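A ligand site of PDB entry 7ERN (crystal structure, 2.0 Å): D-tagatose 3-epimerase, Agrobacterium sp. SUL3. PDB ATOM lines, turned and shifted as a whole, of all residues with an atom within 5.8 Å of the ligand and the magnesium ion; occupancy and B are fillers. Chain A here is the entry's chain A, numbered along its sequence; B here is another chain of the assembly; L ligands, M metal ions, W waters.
OE1 of Glu 150 sits at hydrogen-bond distance from O1 of the ligand, 2.6 Å away.
An oxygen (O6) of the ligand is in hydrogen-bond range of the side-chain hydroxyl (OG) of Ser 64.
The guanidinium group (NH2) of Arg 209 sits close to an oxygen (O2) of the ligand (2.8 Å).
A ring nitrogen (NE2) of His 180 is in hydrogen-bond range of an oxygen (O1) of the ligand, 2.9 Å away.
A ring nitrogen (NE2) of His 7 lies within hydrogen-bond range of an oxygen (O5) of the ligand (3.2 Å).
N of Glu 144 is in hydrogen-bond range of O of Gly 101 (3.0 Å).
OE2 of Glu 238 lies close to NH1 of Arg 209 (3.0 Å).
A ring nitrogen (NE2) of His 175 lies close to a ring nitrogen (NE2) of His 203, 3.5 Å away.
The side-chain carboxylate (OE2) of Glu 36 lies within hydrogen-bond range of the side-chain hydroxyl (OG) of Ser 64, 2.7 Å away.
The backbone carbonyl oxygen of Ser 64 lies within hydrogen-bond range of the backbone NH of Leu 39, at 2.8 Å.
O of Arg 209 is in hydrogen-bond range of N of Phe 240 (3.0 Å).
N of Val 102 lies within hydrogen-bond range of O of Leu 65 (2.9 Å).
O of Thr 100 is in hydrogen-bond range of N of Leu 65.
Residues that only touch the ligand: Val 102 (3.4 Å), Leu 65 (3.6 Å), Val 146 (3.8 Å), Met 9 (3.9 Å), Pro 38 (3.9 Å), Val 66 (3.9 Å) and Gly 101 (3.96 Å).
Hydrophobic or aromatic side chains that line the ligand: His 7, Met 9, Pro 38, Val 66, Val 102, Val 146, His 180 and His 203.
16 residues have an atom within 4 Å of the ligand: His 7, Met 9, Pro 38, Ser 64, Leu 65, Val 66, Gly 101, Val 102, Glu 144, Val 146, Glu 150, Asp 177, His 180, His 203, Arg 209 and Glu 238.
Of the 23 residues printed, 4 come within 4 Å of the magnesium ion.
The magnesium ion is bound by OE2 of Glu 144, at 2.0 Å.
OD2 of Asp 177 is bound to the magnesium ion (2.0 Å).
OE2 of Glu 238 binds the magnesium ion (2.1 Å).
An oxygen (O2) of the ligand is bound to the magnesium ion.
The magnesium ion is bound by ND1 of His 203 (2.2 Å).
The magnesium ion is bound by O3 of the ligand (2.2 Å).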
ATOM      1  N   HIS A   7      31.831  16.274 -16.664  1.00  0.00           N
ATOM      2  CA  HIS A   7      31.898  15.460 -15.473  1.00  0.00           C
ATOM      3  C   HIS A   7      32.644  14.160 -15.769  1.00  0.00           C
ATOM      4  O   HIS A   7      32.424  13.525 -16.808  1.00  0.00           O
ATOM      5  CB  HIS A   7      30.476  15.178 -14.968  1.00  0.00           C
ATOM      6  CG  HIS A   7      30.420  14.677 -13.560  1.00  0.00           C
ATOM      7  ND1 HIS A   7      30.965  13.468 -13.175  1.00  0.00           N
ATOM      8  CD2 HIS A   7      29.863  15.210 -12.440  1.00  0.00           C
ATOM      9  CE1 HIS A   7      30.751  13.278 -11.890  1.00  0.00           C
ATOM     10  NE2 HIS A   7      30.088  14.318 -11.412  1.00  0.00           N
ATOM     11  N   MET A   9      32.301  11.308 -14.700  1.00  0.00           N
ATOM     12  CA  MET A   9      31.398  10.169 -14.855  1.00  0.00           C
ATOM     13  C   MET A   9      31.126   9.813 -16.316  1.00  0.00           C
ATOM     14  O   MET A   9      30.591   8.730 -16.583  1.00  0.00           O
ATOM     15  CB  MET A   9      30.064  10.460 -14.151  1.00  0.00           C
ATOM     16  CG  MET A   9      29.163  11.459 -14.935  1.00  0.00           C
ATOM     17  SD  MET A   9      27.418  11.578 -14.441  1.00  0.00           S
ATOM     18  CE  MET A   9      27.508  12.377 -12.834  1.00  0.00           C
ATOM     19  N   GLU A  36      35.205  17.742 -13.911  1.00  0.00           N
ATOM     20  CA  GLU A  36      34.605  17.658 -12.586  1.00  0.00           C
ATOM     21  C   GLU A  36      34.885  16.260 -12.022  1.00  0.00           C
ATOM     22  O   GLU A  36      34.523  15.251 -12.641  1.00  0.00           O
ATOM     23  CB  GLU A  36      33.113  17.930 -12.621  1.00  0.00           C
ATOM     24  CG  GLU A  36      32.509  17.923 -11.247  1.00  0.00           C
ATOM     25  CD  GLU A  36      31.044  18.287 -11.245  1.00  0.00           C
ATOM     26  OE1 GLU A  36      30.647  19.149 -12.063  1.00  0.00           O
ATOM     27  OE2 GLU A  36      30.282  17.720 -10.431  1.00  0.00           O
ATOM     28  N   PRO A  38      34.466  13.542  -9.098  1.00  0.00           N
ATOM     29  CA  PRO A  38      33.681  13.184  -7.919  1.00  0.00           C
ATOM     30  C   PRO A  38      34.569  12.562  -6.856  1.00  0.00           C
ATOM     31  O   PRO A  38      35.515  11.827  -7.151  1.00  0.00           O
ATOM     32  CB  PRO A  38      32.670  12.170  -8.488  1.00  0.00           C
ATOM     33  CG  PRO A  38      33.471  11.459  -9.553  1.00  0.00           C
ATOM     34  CD  PRO A  38      34.444  12.487 -10.130  1.00  0.00           C
ATOM     35  N   LEU A  39      34.305  12.913  -5.602  1.00  0.00           N
ATOM     36  CA  LEU A  39      34.989  12.332  -4.455  1.00  0.00           C
ATOM     37  C   LEU A  39      34.001  11.437  -3.709  1.00  0.00           C
ATOM     38  O   LEU A  39      33.074  11.933  -3.055  1.00  0.00           O
ATOM     39  CB  LEU A  39      35.528  13.422  -3.519  1.00  0.00           C
ATOM     40  CG  LEU A  39      36.456  14.469  -4.136  1.00  0.00           C
ATOM     41  CD1 LEU A  39      36.729  15.555  -3.130  1.00  0.00           C
ATOM     42  CD2 LEU A  39      37.753  13.836  -4.602  1.00  0.00           C
ATOM     43  N   SER A  64      33.497  17.332  -6.728  1.00  0.00           N
ATOM     44  CA  SER A  64      32.116  17.311  -6.284  1.00  0.00           C
ATOM     45  C   SER A  64      31.846  16.066  -5.439  1.00  0.00           C
ATOM     46  O   SER A  64      32.590  15.082  -5.480  1.00  0.00           O
ATOM     47  CB  SER A  64      31.115  17.374  -7.457  1.00  0.00           C
ATOM     48  OG  SER A  64      31.249  16.262  -8.322  1.00  0.00           O
ATOM     49  N   LEU A  65      30.747  16.111  -4.696  1.00  0.00           N
ATOM     50  CA  LEU A  65      30.347  14.970  -3.898  1.00  0.00           C
ATOM     51  C   LEU A  65      28.881  15.088  -3.530  1.00  0.00           C
ATOM     52  O   LEU A  65      28.233  16.131  -3.693  1.00  0.00           O
ATOM     53  CB  LEU A  65      31.190  14.848  -2.617  1.00  0.00           C
ATOM     54  CG  LEU A  65      31.286  15.998  -1.586  1.00  0.00           C
ATOM     55  CD1 LEU A  65      29.998  16.297  -0.810  1.00  0.00           C
ATOM     56  CD2 LEU A  65      32.388  15.634  -0.590  1.00  0.00           C
ATOM     57  N   VAL A  66      28.368  13.972  -3.031  1.00  0.00           N
ATOM     58  CA  VAL A  66      27.129  13.872  -2.263  1.00  0.00           C
ATOM     59  C   VAL A  66      27.515  13.402  -0.862  1.00  0.00           C
ATOM     60  O   VAL A  66      28.326  12.486  -0.718  1.00  0.00           O
ATOM     61  CB  VAL A  66      26.167  12.871  -2.928  1.00  0.00           C
ATOM     62  CG1 VAL A  66      24.906  12.716  -2.105  1.00  0.00           C
ATOM     63  CG2 VAL A  66      25.830  13.293  -4.372  1.00  0.00           C
ATOM     64  N   THR A 100      31.942  21.273  -4.989  1.00  0.00           N
ATOM     65  CA  THR A 100      30.535  21.575  -5.219  1.00  0.00           C
ATOM     66  C   THR A 100      29.732  20.272  -5.173  1.00  0.00           C
ATOM     67  O   THR A 100      30.246  19.225  -4.766  1.00  0.00           O
ATOM     68  CB  THR A 100      30.380  22.330  -6.557  1.00  0.00           C
ATOM     69  OG1 THR A 100      29.049  22.807  -6.693  1.00  0.00           O
ATOM     70  CG2 THR A 100      30.707  21.417  -7.735  1.00  0.00           C
ATOM     71  N   GLY A 101      28.483  20.334  -5.604  1.00  0.00           N
ATOM     72  CA  GLY A 101      27.594  19.183  -5.580  1.00  0.00           C
ATOM     73  C   GLY A 101      26.595  19.265  -4.440  1.00  0.00           C
ATOM     74  O   GLY A 101      26.237  20.339  -3.960  1.00  0.00           O
ATOM     75  N   VAL A 102      26.133  18.084  -4.015  1.00  0.00           N
ATOM     76  CA  VAL A 102      25.172  18.058  -2.918  1.00  0.00           C
ATOM     77  C   VAL A 102      25.960  18.042  -1.621  1.00  0.00           C
ATOM     78  O   VAL A 102      26.076  17.015  -0.942  1.00  0.00           O
ATOM     79  CB  VAL A 102      24.199  16.872  -3.060  1.00  0.00           C
ATOM     80  CG1 VAL A 102      23.063  16.979  -2.048  1.00  0.00           C
ATOM     81  CG2 VAL A 102      23.612  16.877  -4.489  1.00  0.00           C
ATOM     82  N   THR A 107      21.305  12.500  -1.899  1.00  0.00           N
ATOM     83  CA  THR A 107      20.428  12.411  -3.047  1.00  0.00           C
ATOM     84  C   THR A 107      19.394  11.308  -2.888  1.00  0.00           C
ATOM     85  O   THR A 107      18.615  11.043  -3.813  1.00  0.00           O
ATOM     86  CB  THR A 107      21.267  12.182  -4.308  1.00  0.00           C
ATOM     87  OG1 THR A 107      22.188  11.127  -4.067  1.00  0.00           O
ATOM     88  CG2 THR A 107      22.041  13.465  -4.643  1.00  0.00           C
ATOM     89  N   GLU A 144      24.661  22.762  -4.880  1.00  0.00           N
ATOM     90  CA  GLU A 144      23.883  22.336  -6.046  1.00  0.00           C
ATOM     91  C   GLU A 144      22.446  22.009  -5.630  1.00  0.00           C
ATOM     92  O   GLU A 144      22.219  21.086  -4.841  1.00  0.00           O
ATOM     93  CB  GLU A 144      24.506  21.134  -6.755  1.00  0.00           C
ATOM     94  CG  GLU A 144      23.691  20.669  -8.008  1.00  0.00           C
ATOM     95  CD  GLU A 144      24.301  19.484  -8.740  1.00  0.00           C
ATOM     96  OE1 GLU A 144      25.360  18.977  -8.289  1.00  0.00           O
ATOM     97  OE2 GLU A 144      23.711  19.029  -9.772  1.00  0.00           O
ATOM     98  N   VAL A 146      19.006  20.229  -6.110  1.00  0.00           N
ATOM     99  CA  VAL A 146      18.565  19.001  -6.740  1.00  0.00           C
ATOM    100  C   VAL A 146      17.056  18.882  -6.587  1.00  0.00           C
ATOM    101  O   VAL A 146      16.433  19.642  -5.860  1.00  0.00           O
ATOM    102  CB  VAL A 146      19.289  17.769  -6.177  1.00  0.00           C
ATOM    103  CG1 VAL A 146      20.788  17.884  -6.421  1.00  0.00           C
ATOM    104  CG2 VAL A 146      19.007  17.625  -4.672  1.00  0.00           C
ATOM    105  N   GLU A 150      15.278  13.756  -4.631  1.00  0.00           N
ATOM    106  CA  GLU A 150      16.596  13.432  -4.118  1.00  0.00           C
ATOM    107  C   GLU A 150      16.840  14.050  -2.751  1.00  0.00           C
ATOM    108  O   GLU A 150      17.633  13.506  -1.955  1.00  0.00           O
ATOM    109  CB  GLU A 150      17.665  13.925  -5.107  1.00  0.00           C
ATOM    110  CG  GLU A 150      17.588  13.171  -6.420  1.00  0.00           C
ATOM    111  CD  GLU A 150      18.790  13.413  -7.302  1.00  0.00           C
ATOM    112  OE1 GLU A 150      19.699  14.162  -6.865  1.00  0.00           O
ATOM    113  OE2 GLU A 150      18.832  12.858  -8.420  1.00  0.00           O
ATOM    114  N   HIS A 175      25.042  26.490  -7.577  1.00  0.00           N
ATOM    115  CA  HIS A 175      25.318  25.554  -8.660  1.00  0.00           C
ATOM    116  C   HIS A 175      23.965  25.004  -9.079  1.00  0.00           C
ATOM    117  O   HIS A 175      23.266  24.407  -8.251  1.00  0.00           O
ATOM    118  CB  HIS A 175      26.275  24.457  -8.142  1.00  0.00           C
ATOM    119  CG  HIS A 175      26.492  23.288  -9.049  1.00  0.00           C
ATOM    120  ND1 HIS A 175      27.359  22.267  -8.731  1.00  0.00           N
ATOM    121  CD2 HIS A 175      25.957  22.961 -10.253  1.00  0.00           C
ATOM    122  CE1 HIS A 175      27.348  21.355  -9.689  1.00  0.00           C
ATOM    123  NE2 HIS A 175      26.502  21.759 -10.630  1.00  0.00           N
ATOM    124  N   ASP A 177      21.460  22.774 -11.901  1.00  0.00           N
ATOM    125  CA  ASP A 177      21.503  21.591 -12.759  1.00  0.00           C
ATOM    126  C   ASP A 177      20.231  21.597 -13.590  1.00  0.00           C
ATOM    127  O   ASP A 177      19.133  21.586 -13.020  1.00  0.00           O
ATOM    128  CB  ASP A 177      21.649  20.320 -11.911  1.00  0.00           C
ATOM    129  CG  ASP A 177      21.721  19.044 -12.756  1.00  0.00           C
ATOM    130  OD1 ASP A 177      21.042  18.969 -13.798  1.00  0.00           O
ATOM    131  OD2 ASP A 177      22.448  18.098 -12.357  1.00  0.00           O
ATOM    132  N   HIS A 180      17.584  18.992 -12.896  1.00  0.00           N
ATOM    133  CA  HIS A 180      16.766  19.251 -11.722  1.00  0.00           C
ATOM    134  C   HIS A 180      15.865  20.460 -11.914  1.00  0.00           C
ATOM    135  O   HIS A 180      14.715  20.469 -11.451  1.00  0.00           O
ATOM    136  CB  HIS A 180      17.672  19.450 -10.520  1.00  0.00           C
ATOM    137  CG  HIS A 180      18.479  18.230 -10.170  1.00  0.00           C
ATOM    138  ND1 HIS A 180      17.891  17.012  -9.898  1.00  0.00           N
ATOM    139  CD2 HIS A 180      19.811  18.057 -10.035  1.00  0.00           C
ATOM    140  CE1 HIS A 180      18.840  16.133  -9.619  1.00  0.00           C
ATOM    141  NE2 HIS A 180      20.014  16.735  -9.691  1.00  0.00           N
ATOM    142  N   HIS A 203      25.436  22.450 -14.140  1.00  0.00           N
ATOM    143  CA  HIS A 203      25.384  21.156 -14.799  1.00  0.00           C
ATOM    144  C   HIS A 203      24.426  21.281 -15.977  1.00  0.00           C
ATOM    145  O   HIS A 203      23.227  21.506 -15.801  1.00  0.00           O
ATOM    146  CB  HIS A 203      24.956  20.050 -13.844  1.00  0.00           C
ATOM    147  CG  HIS A 203      26.092  19.515 -13.016  1.00  0.00           C
ATOM    148  ND1 HIS A 203      25.899  18.674 -11.946  1.00  0.00           N
ATOM    149  CD2 HIS A 203      27.431  19.713 -13.117  1.00  0.00           C
ATOM    150  CE1 HIS A 203      27.086  18.373 -11.421  1.00  0.00           C
ATOM    151  NE2 HIS A 203      28.016  18.991 -12.112  1.00  0.00           N
ATOM    152  N   ARG A 209      18.805  12.844 -18.618  1.00  0.00           N
ATOM    153  CA  ARG A 209      20.214  12.578 -18.355  1.00  0.00           C
ATOM    154  C   ARG A 209      20.906  11.992 -19.569  1.00  0.00           C
ATOM    155  O   ARG A 209      21.991  11.425 -19.439  1.00  0.00           O
ATOM    156  CB  ARG A 209      20.415  11.642 -17.147  1.00  0.00           C
ATOM    157  CG  ARG A 209      19.951  12.244 -15.820  1.00  0.00           C
ATOM    158  CD  ARG A 209      20.857  13.407 -15.419  1.00  0.00           C
ATOM    159  NE  ARG A 209      20.850  13.620 -13.986  1.00  0.00           N
ATOM    160  CZ  ARG A 209      21.349  14.700 -13.377  1.00  0.00           C
ATOM    161  NH1 ARG A 209      21.895  15.684 -14.091  1.00  0.00           N
ATOM    162  NH2 ARG A 209      21.315  14.791 -12.049  1.00  0.00           N
ATOM    163  N   GLU A 238      26.763  16.994 -17.748  1.00  0.00           N
ATOM    164  CA  GLU A 238      26.474  15.837 -16.901  1.00  0.00           C
ATOM    165  C   GLU A 238      25.495  14.946 -17.641  1.00  0.00           C
ATOM    166  O   GLU A 238      24.414  15.398 -18.037  1.00  0.00           O
ATOM    167  CB  GLU A 238      25.908  16.294 -15.548  1.00  0.00           C
ATOM    168  CG  GLU A 238      25.369  15.174 -14.652  1.00  0.00           C
ATOM    169  CD  GLU A 238      25.354  15.605 -13.194  1.00  0.00           C
ATOM    170  OE1 GLU A 238      26.266  15.203 -12.435  1.00  0.00           O
ATOM    171  OE2 GLU A 238      24.461  16.385 -12.807  1.00  0.00           O
ATOM    172  N   PHE A 240      24.332  10.466 -17.872  1.00  0.00           N
ATOM    173  CA  PHE A 240      24.514   9.141 -17.276  1.00  0.00           C
ATOM    174  C   PHE A 240      24.886   8.066 -18.303  1.00  0.00           C
ATOM    175  O   PHE A 240      24.859   6.871 -17.977  1.00  0.00           O
ATOM    176  CB  PHE A 240      23.262   8.738 -16.488  1.00  0.00           C
ATOM    177  CG  PHE A 240      23.079   9.491 -15.192  1.00  0.00           C
ATOM    178  CD1 PHE A 240      24.052  10.353 -14.720  1.00  0.00           C
ATOM    179  CD2 PHE A 240      21.929   9.306 -14.430  1.00  0.00           C
ATOM    180  CE1 PHE A 240      23.876  11.043 -13.508  1.00  0.00           C
ATOM    181  CE2 PHE A 240      21.750   9.991 -13.242  1.00  0.00           C
ATOM    182  CZ  PHE A 240      22.731  10.851 -12.775  1.00  0.00           C
ATOM    183  N   TYR B 149      11.957   8.037 -10.087  1.00  0.00           N
ATOM    184  CA  TYR B 149      12.057   8.189  -8.639  1.00  0.00           C
ATOM    185  C   TYR B 149      10.863   7.589  -7.897  1.00  0.00           C
ATOM    186  O   TYR B 149      10.965   7.338  -6.682  1.00  0.00           O
ATOM    187  CB  TYR B 149      12.170   9.659  -8.271  1.00  0.00           C
ATOM    188  CG  TYR B 149      13.450  10.311  -8.699  1.00  0.00           C
ATOM    189  CD1 TYR B 149      14.629  10.155  -7.957  1.00  0.00           C
ATOM    190  CD2 TYR B 149      13.482  11.112  -9.844  1.00  0.00           C
ATOM    191  CE1 TYR B 149      15.799  10.777  -8.344  1.00  0.00           C
ATOM    192  CE2 TYR B 149      14.647  11.737 -10.238  1.00  0.00           C
ATOM    193  CZ  TYR B 149      15.788  11.567  -9.479  1.00  0.00           C
ATOM    194  OH  TYR B 149      16.945  12.185  -9.883  1.00  0.00           O
HETATM  195  C1  LIG L   1      23.045  14.369  -8.576  1.00  0.00           C
HETATM  196  C2  LIG L   1      23.722  15.383  -9.489  1.00  0.00           C
HETATM  197  C3  LIG L   1      25.232  15.554  -9.445  1.00  0.00           C
HETATM  198  C4  LIG L   1      25.887  15.162  -8.128  1.00  0.00           C
HETATM  199  C5  LIG L   1      27.392  15.102  -8.393  1.00  0.00           C
HETATM  200  C6  LIG L   1      28.213  14.720  -7.156  1.00  0.00           C
HETATM  201  O1  LIG L   1      21.736  14.815  -8.423  1.00  0.00           O
HETATM  202  O2  LIG L   1      23.086  16.030 -10.271  1.00  0.00           O
HETATM  203  O3  LIG L   1      25.456  16.920  -9.652  1.00  0.00           O
HETATM  204  O4  LIG L   1      25.622  16.136  -7.170  1.00  0.00           O
HETATM  205  O5  LIG L   1      27.586  14.167  -9.417  1.00  0.00           O
HETATM  206  O6  LIG L   1      29.493  14.242  -7.518  1.00  0.00           O
HETATM  207 MG    MG M   1      24.080  17.688 -11.227  1.00  0.00          MG
HETATM  208  O   HOH W   1      26.170  11.465  -9.356  1.00  0.00           O
HETATM  209  O   HOH W   2      30.101  12.061  -6.513  1.00  0.00           O
